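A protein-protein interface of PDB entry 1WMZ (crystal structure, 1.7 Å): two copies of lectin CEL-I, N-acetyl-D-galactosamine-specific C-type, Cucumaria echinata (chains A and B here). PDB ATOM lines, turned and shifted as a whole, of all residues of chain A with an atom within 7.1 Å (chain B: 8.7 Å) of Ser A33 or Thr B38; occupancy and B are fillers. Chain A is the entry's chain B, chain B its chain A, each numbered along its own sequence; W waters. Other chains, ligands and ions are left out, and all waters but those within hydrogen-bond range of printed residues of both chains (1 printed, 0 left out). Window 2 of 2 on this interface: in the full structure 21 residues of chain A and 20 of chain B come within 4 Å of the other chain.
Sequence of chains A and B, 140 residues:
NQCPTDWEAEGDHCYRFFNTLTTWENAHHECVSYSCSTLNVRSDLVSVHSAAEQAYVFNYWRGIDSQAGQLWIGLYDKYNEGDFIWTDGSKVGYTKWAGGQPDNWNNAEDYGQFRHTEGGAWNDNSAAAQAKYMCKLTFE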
ATOM      1  N   PRO A   4      12.327   0.152   8.450  1.00  0.00           N
ATOM      2  CA  PRO A   4      11.980   1.076   7.363  1.00  0.00           C
ATOM      3  C   PRO A   4      12.693   0.745   6.082  1.00  0.00           C
ATOM      4  O   PRO A   4      13.752   0.105   6.081  1.00  0.00           O
ATOM      5  CB  PRO A   4      12.427   2.436   7.898  1.00  0.00           C
ATOM      6  CG  PRO A   4      12.353   2.265   9.426  1.00  0.00           C
ATOM      7  CD  PRO A   4      12.826   0.854   9.654  1.00  0.00           C
ATOM      8  N   TRP A   7      16.628   0.479   5.100  1.00  0.00           N
ATOM      9  CA  TRP A   7      17.343   0.036   6.278  1.00  0.00           C
ATOM     10  C   TRP A   7      17.333  -1.483   6.335  1.00  0.00           C
ATOM     11  O   TRP A   7      16.426  -2.129   5.785  1.00  0.00           O
ATOM     12  CB  TRP A   7      16.703   0.595   7.559  1.00  0.00           C
ATOM     13  CG  TRP A   7      16.746   2.092   7.670  1.00  0.00           C
ATOM     14  CD1 TRP A   7      16.046   2.974   6.937  1.00  0.00           C
ATOM     15  CD2 TRP A   7      17.537   2.867   8.582  1.00  0.00           C
ATOM     16  NE1 TRP A   7      16.359   4.264   7.291  1.00  0.00           N
ATOM     17  CE2 TRP A   7      17.259   4.232   8.319  1.00  0.00           C
ATOM     18  CE3 TRP A   7      18.434   2.557   9.595  1.00  0.00           C
ATOM     19  CZ2 TRP A   7      17.849   5.282   9.041  1.00  0.00           C
ATOM     20  CZ3 TRP A   7      19.040   3.602  10.292  1.00  0.00           C
ATOM     21  CH2 TRP A   7      18.741   4.955   9.995  1.00  0.00           C
ATOM     22  N   ARG A  16      21.729   1.379   8.420  1.00  0.00           N
ATOM     23  CA  ARG A  16      21.700   1.925   7.086  1.00  0.00           C
ATOM     24  C   ARG A  16      23.033   2.551   6.741  1.00  0.00           C
ATOM     25  O   ARG A  16      23.533   3.478   7.443  1.00  0.00           O
ATOM     26  CB  ARG A  16      20.625   2.998   6.936  1.00  0.00           C
ATOM     27  CG  ARG A  16      20.473   3.517   5.516  1.00  0.00           C
ATOM     28  CD  ARG A  16      19.187   4.264   5.223  1.00  0.00           C
ATOM     29  NE  ARG A  16      19.152   4.756   3.836  1.00  0.00           N
ATOM     30  CZ  ARG A  16      18.204   5.567   3.358  1.00  0.00           C
ATOM     31  NH1 ARG A  16      17.175   5.934   4.106  1.00  0.00           N
ATOM     32  NH2 ARG A  16      18.268   6.008   2.126  1.00  0.00           N
ATOM     33  N   ALA A  27      27.912  13.560   9.530  1.00  0.00           N
ATOM     34  CA  ALA A  27      27.402  12.218   9.641  1.00  0.00           C
ATOM     35  C   ALA A  27      26.552  12.021  10.892  1.00  0.00           C
ATOM     36  O   ALA A  27      25.521  11.357  10.844  1.00  0.00           O
ATOM     37  CB  ALA A  27      28.532  11.194   9.598  1.00  0.00           C
ATOM     38  N   HIS A  28      27.013  12.540  12.018  1.00  0.00           N
ATOM     39  CA  HIS A  28      26.277  12.476  13.233  1.00  0.00           C
ATOM     40  C   HIS A  28      24.865  13.092  13.073  1.00  0.00           C
ATOM     41  O   HIS A  28      23.848  12.439  13.397  1.00  0.00           O
ATOM     42  CB  HIS A  28      27.032  13.193  14.363  1.00  0.00           C
ATOM     43  CG  HIS A  28      26.467  12.912  15.725  1.00  0.00           C
ATOM     44  ND1 HIS A  28      26.934  13.535  16.858  1.00  0.00           N
ATOM     45  CD2 HIS A  28      25.408  12.177  16.117  1.00  0.00           C
ATOM     46  CE1 HIS A  28      26.250  13.118  17.907  1.00  0.00           C
ATOM     47  NE2 HIS A  28      25.327  12.274  17.494  1.00  0.00           N
ATOM     48  N   HIS A  29      24.799  14.344  12.593  1.00  0.00           N
ATOM     49  CA  HIS A  29      23.553  15.034  12.347  1.00  0.00           C
ATOM     50  C   HIS A  29      22.692  14.197  11.343  1.00  0.00           C
ATOM     51  O   HIS A  29      21.499  13.965  11.577  1.00  0.00           O
ATOM     52  CB  HIS A  29      23.783  16.454  11.796  1.00  0.00           C
ATOM     53  CG  HIS A  29      24.124  17.462  12.853  1.00  0.00           C
ATOM     54  ND1 HIS A  29      23.194  17.934  13.743  1.00  0.00           N
ATOM     55  CD2 HIS A  29      25.298  18.066  13.172  1.00  0.00           C
ATOM     56  CE1 HIS A  29      23.791  18.748  14.609  1.00  0.00           C
ATOM     57  NE2 HIS A  29      25.069  18.849  14.274  1.00  0.00           N
ATOM     58  N   GLU A  30      23.286  13.743  10.240  1.00  0.00           N
ATOM     59  CA  GLU A  30      22.488  12.998   9.248  1.00  0.00           C
ATOM     60  C   GLU A  30      21.819  11.791   9.920  1.00  0.00           C
ATOM     61  O   GLU A  30      20.611  11.533   9.699  1.00  0.00           O
ATOM     62  CB  GLU A  30      23.350  12.486   8.100  1.00  0.00           C
ATOM     63  CG  GLU A  30      23.755  13.556   7.094  1.00  0.00           C
ATOM     64  CD  GLU A  30      22.579  14.143   6.352  1.00  0.00           C
ATOM     65  OE1 GLU A  30      22.616  15.366   6.135  1.00  0.00           O
ATOM     66  OE2 GLU A  30      21.630  13.424   5.979  1.00  0.00           O
ATOM     67  N   CYS A  31      22.568  11.070  10.751  1.00  0.00           N
ATOM     68  CA  CYS A  31      22.011   9.868  11.362  1.00  0.00           C
ATOM     69  C   CYS A  31      20.918  10.249  12.345  1.00  0.00           C
ATOM     70  O   CYS A  31      19.843   9.639  12.320  1.00  0.00           O
ATOM     71  CB  CYS A  31      23.039   9.003  12.081  1.00  0.00           C
ATOM     72  SG  CYS A  31      24.175   8.124  11.005  1.00  0.00           S
ATOM     73  N   VAL A  32      21.133  11.298  13.154  1.00  0.00           N
ATOM     74  CA  VAL A  32      20.117  11.683  14.157  1.00  0.00           C
ATOM     75  C   VAL A  32      18.838  12.165  13.459  1.00  0.00           C
ATOM     76  O   VAL A  32      17.738  11.995  13.975  1.00  0.00           O
ATOM     77  CB  VAL A  32      20.679  12.712  15.139  1.00  0.00           C
ATOM     78  CG1 VAL A  32      19.578  13.243  16.049  1.00  0.00           C
ATOM     79  CG2 VAL A  32      21.817  12.087  15.988  1.00  0.00           C
ATOM     80  N   SER A  33      18.963  12.673  12.225  1.00  0.00           N
ATOM     81  CA  SER A  33      17.827  13.179  11.467  1.00  0.00           C
ATOM     82  C   SER A  33      16.791  12.133  11.126  1.00  0.00           C
ATOM     83  O   SER A  33      15.667  12.522  10.760  1.00  0.00           O
ATOM     84  CB  SER A  33      18.300  13.876  10.190  1.00  0.00           C
ATOM     85  OG  SER A  33      18.490  13.010   9.103  1.00  0.00           O
ATOM     86  N   TYR A  34      17.140  10.840  11.252  1.00  0.00           N
ATOM     87  CA  TYR A  34      16.179   9.743  10.956  1.00  0.00           C
ATOM     88  C   TYR A  34      15.404   9.317  12.218  1.00  0.00           C
ATOM     89  O   TYR A  34      14.667   8.337  12.172  1.00  0.00           O
ATOM     90  CB  TYR A  34      16.875   8.544  10.307  1.00  0.00           C
ATOM     91  CG  TYR A  34      17.436   8.884   8.966  1.00  0.00           C
ATOM     92  CD1 TYR A  34      18.788   9.185   8.821  1.00  0.00           C
ATOM     93  CD2 TYR A  34      16.637   8.928   7.836  1.00  0.00           C
ATOM     94  CE1 TYR A  34      19.297   9.564   7.618  1.00  0.00           C
ATOM     95  CE2 TYR A  34      17.161   9.282   6.599  1.00  0.00           C
ATOM     96  CZ  TYR A  34      18.484   9.617   6.498  1.00  0.00           C
ATOM     97  OH  TYR A  34      19.049   9.970   5.271  1.00  0.00           O
ATOM     98  N   SER A  35      15.565  10.050  13.321  1.00  0.00           N
ATOM     99  CA  SER A  35      14.804   9.736  14.531  1.00  0.00           C
ATOM    100  C   SER A  35      13.316  10.022  14.340  1.00  0.00           C
ATOM    101  O   SER A  35      12.898  10.898  13.547  1.00  0.00           O
ATOM    102  CB  SER A  35      15.282  10.527  15.758  1.00  0.00           C
ATOM    103  OG  SER A  35      16.679  10.384  16.011  1.00  0.00           O
ATOM    104  N   CYS A  36      12.514   9.272  15.102  1.00  0.00           N
ATOM    105  CA  CYS A  36      11.050   9.389  15.037  1.00  0.00           C
ATOM    106  C   CYS A  36      10.507   9.479  16.442  1.00  0.00           C
ATOM    107  O   CYS A  36      10.330   8.438  17.050  1.00  0.00           O
ATOM    108  CB  CYS A  36      10.492   8.164  14.378  1.00  0.00           C
ATOM    109  SG  CYS A  36      10.703   8.111  12.596  1.00  0.00           S
ATOM    110  N   SER A  37      10.250  10.680  16.948  1.00  0.00           N
ATOM    111  CA  SER A  37       9.798  10.846  18.354  1.00  0.00           C
ATOM    112  C   SER A  37       8.449  10.194  18.623  1.00  0.00           C
ATOM    113  O   SER A  37       8.189   9.718  19.727  1.00  0.00           O
ATOM    114  CB  SER A  37       9.700  12.324  18.767  1.00  0.00           C
ATOM    115  OG  SER A  37       8.739  13.054  17.989  1.00  0.00           O
ATOM    116  N   SER A  43      17.608   7.496  16.237  1.00  0.00           N
ATOM    117  CA  SER A  43      18.578   7.150  15.196  1.00  0.00           C
ATOM    118  C   SER A  43      19.877   7.855  15.541  1.00  0.00           C
ATOM    119  O   SER A  43      19.872   8.988  15.998  1.00  0.00           O
ATOM    120  CB  SER A  43      18.110   7.592  13.819  1.00  0.00           C
ATOM    121  OG  SER A  43      19.051   7.139  12.854  1.00  0.00           O
ATOM    122  N   ASP A  44      20.985   7.150  15.349  1.00  0.00           N
ATOM    123  CA  ASP A  44      22.291   7.701  15.672  1.00  0.00           C
ATOM    124  C   ASP A  44      23.356   7.051  14.814  1.00  0.00           C
ATOM    125  O   ASP A  44      23.094   6.077  14.058  1.00  0.00           O
ATOM    126  CB  ASP A  44      22.542   7.440  17.161  1.00  0.00           C
ATOM    127  CG  ASP A  44      23.451   8.452  17.834  1.00  0.00           C
ATOM    128  OD1 ASP A  44      23.216   8.760  19.064  1.00  0.00           O
ATOM    129  OD2 ASP A  44      24.389   9.024  17.243  1.00  0.00           O
ATOM    130  N   SER B  35       2.540   8.447  12.769  1.00  0.00           N
ATOM    131  CA  SER B  35       3.361   8.334  11.556  1.00  0.00           C
ATOM    132  C   SER B  35       4.660   9.127  11.688  1.00  0.00           C
ATOM    133  O   SER B  35       4.728  10.151  12.373  1.00  0.00           O
ATOM    134  CB  SER B  35       2.614   8.829  10.323  1.00  0.00           C
ATOM    135  OG  SER B  35       1.358   8.161  10.149  1.00  0.00           O
ATOM    136  N   CYS B  36       5.655   8.698  10.924  1.00  0.00           N
ATOM    137  CA  CYS B  36       6.958   9.360  10.955  1.00  0.00           C
ATOM    138  C   CYS B  36       7.552   9.487   9.548  1.00  0.00           C
ATOM    139  O   CYS B  36       8.054   8.514   8.953  1.00  0.00           O
ATOM    140  CB  CYS B  36       7.889   8.627  11.860  1.00  0.00           C
ATOM    141  SG  CYS B  36       9.458   9.492  11.835  1.00  0.00           S
ATOM    142  N   SER B  37       7.540  10.715   9.056  1.00  0.00           N
ATOM    143  CA  SER B  37       8.012  11.013   7.713  1.00  0.00           C
ATOM    144  C   SER B  37       9.530  10.794   7.551  1.00  0.00           C
ATOM    145  O   SER B  37       9.976  10.448   6.472  1.00  0.00           O
ATOM    146  CB  SER B  37       7.618  12.435   7.341  1.00  0.00           C
ATOM    147  OG  SER B  37       7.870  12.657   5.947  1.00  0.00           O
ATOM    148  N   THR B  38      10.337  11.026   8.586  1.00  0.00           N
ATOM    149  CA  THR B  38      11.776  10.846   8.423  1.00  0.00           C
ATOM    150  C   THR B  38      12.177   9.407   8.102  1.00  0.00           C
ATOM    151  O   THR B  38      13.237   9.184   7.513  1.00  0.00           O
ATOM    152  CB  THR B  38      12.558  11.261   9.685  1.00  0.00           C
ATOM    153  OG1 THR B  38      12.016  10.560  10.820  1.00  0.00           O
ATOM    154  CG2 THR B  38      12.459  12.707   9.952  1.00  0.00           C
ATOM    155  N   LEU B  39      11.360   8.428   8.478  1.00  0.00           N
ATOM    156  CA  LEU B  39      11.637   7.024   8.148  1.00  0.00           C
ATOM    157  C   LEU B  39      10.605   6.460   7.136  1.00  0.00           C
ATOM    158  O   LEU B  39      10.595   5.266   6.885  1.00  0.00           O
ATOM    159  CB  LEU B  39      11.609   6.173   9.410  1.00  0.00           C
ATOM    160  CG  LEU B  39      12.855   6.389  10.300  1.00  0.00           C
ATOM    161  CD1 LEU B  39      12.750   5.705  11.630  1.00  0.00           C
ATOM    162  CD2 LEU B  39      14.086   5.961   9.578  1.00  0.00           C
ATOM    163  N   ASN B  40       9.739   7.327   6.608  1.00  0.00           N
ATOM    164  CA  ASN B  40       8.588   6.920   5.762  1.00  0.00           C
ATOM    165  C   ASN B  40       7.780   5.805   6.380  1.00  0.00           C
ATOM    166  O   ASN B  40       7.449   4.796   5.713  1.00  0.00           O
ATOM    167  CB  ASN B  40       9.078   6.504   4.374  1.00  0.00           C
ATOM    168  CG  ASN B  40       9.877   7.583   3.745  1.00  0.00           C
ATOM    169  OD1 ASN B  40       9.344   8.638   3.449  1.00  0.00           O
ATOM    170  ND2 ASN B  40      11.194   7.371   3.647  1.00  0.00           N
ATOM    171  N   VAL B  41       7.521   5.951   7.677  1.00  0.00           N
ATOM    172  CA  VAL B  41       6.637   5.050   8.388  1.00  0.00           C
ATOM    173  C   VAL B  41       5.218   5.639   8.442  1.00  0.00           C
ATOM    174  O   VAL B  41       4.946   6.630   9.126  1.00  0.00           O
ATOM    175  CB  VAL B  41       7.122   4.751   9.825  1.00  0.00           C
ATOM    176  CG1 VAL B  41       6.216   3.749  10.457  1.00  0.00           C
ATOM    177  CG2 VAL B  41       8.598   4.216   9.864  1.00  0.00           C
ATOM    178  N   ARG B  42       4.297   4.998   7.738  1.00  0.00           N
ATOM    179  CA  ARG B  42       2.872   5.244   7.896  1.00  0.00           C
ATOM    180  C   ARG B  42       2.300   4.490   9.101  1.00  0.00           C
ATOM    181  O   ARG B  42       2.515   3.271   9.252  1.00  0.00           O
ATOM    182  CB  ARG B  42       2.102   4.782   6.669  1.00  0.00           C
ATOM    183  CG  ARG B  42       0.548   4.822   6.854  1.00  0.00           C
ATOM    184  CD  ARG B  42      -0.254   4.406   5.618  1.00  0.00           C
ATOM    185  NE  ARG B  42      -0.078   5.374   4.533  1.00  0.00           N
ATOM    186  CZ  ARG B  42      -0.801   6.448   4.362  1.00  0.00           C
ATOM    187  NH1 ARG B  42      -1.851   6.695   5.137  1.00  0.00           N
ATOM    188  NH2 ARG B  42      -0.514   7.292   3.373  1.00  0.00           N
HETATM  189  O   HOH W   1       7.915  10.496  14.755  1.00  0.00           O
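The backbone carbonyl oxygen of Val B41 sits at hydrogen-bond distance from the backbone NH of Cys B36 (2.8 Å).
The backbone NH of Ser A43 lies within hydrogen-bond range of the side-chain hydroxyl of Ser A35, at 3.0 Å.
The backbone carbonyl oxygen (O) of Glu A30 lies within hydrogen-bond range of the side-chain hydroxyl (OG) of Ser A33.
O of Val A32 sits at hydrogen-bond distance from OG of Ser A35, at 2.8 Å.
SG of Cys B36 is in hydrogen-bond range of OG1 of Thr B38, at 3.0 Å.
Cys A36 touches its own counterpart, Cys B36.
Of the 9 pairs that touch across the chains among the printed residues, 1 has its exchanged pair printed and touching as well.
Water W1 lies within hydrogen-bond range of N of Ser A37 (3.2 Å) and SG of Cys B36 (3.5 Å).
Of the 8 printed residues of chain B, 3 touch a printed residue of chain A.
Hydrophobic or aromatic side chains of chain B that line the printed part of chain A: Leu B39.
Pro A4 touches Leu B39 (CB to O, 3.5 Å).
Trp A7 touches Leu B39.
Thr B38 touches Ser A33.
Thr B38 touches Tyr A34.
O of Tyr A34 touches CG of Leu B39, at 3.3 Å.
SG of Cys A36 touches CD1 of Leu B39, 3.3 Å away.
Of chain B, only Thr B38 comes within 4 Å of Ser A33.
Of chain A, only Ser A33 (3.3 Å), Tyr A34 (3.4 Å), Ser A35 (2.9 Å) and Cys A36 (3.3 Å) come within 4 Å of Thr B38.
Of the printed residues of chain A, Cys B36 touches Cys A36 (2.0 Å).
Printed residues of chain B within 4 Å of Cys A36: Cys B36 (2.0 Å), Thr B38 (3.3 Å) and Leu B39 (3.3 Å).
Of the printed residues of chain B, Ser A35 touches Thr B38.
Of the printed residues of chain B, Pro A4 touches Leu B39 (3.5 Å).
Of the printed residues of chain B, Tyr A34 touches Thr B38 and Leu B39.
The nearest residue of chain B that does not touch Ser A33 is Leu B39 (6.4 Å).
The nearest residue of chain A that does not touch Thr B38 is Trp A7 (5.8 Å).
SG of Cys A36 sits at hydrogen-bond distance from OG1 of Thr B38.
The side-chain sulfur of Cys B36 forms a disulfide with the side-chain sulfur of Cys A36 (2.0 Å).
OG1 of Thr B38 is in hydrogen-bond range of O of Ser A35 (2.9 Å).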
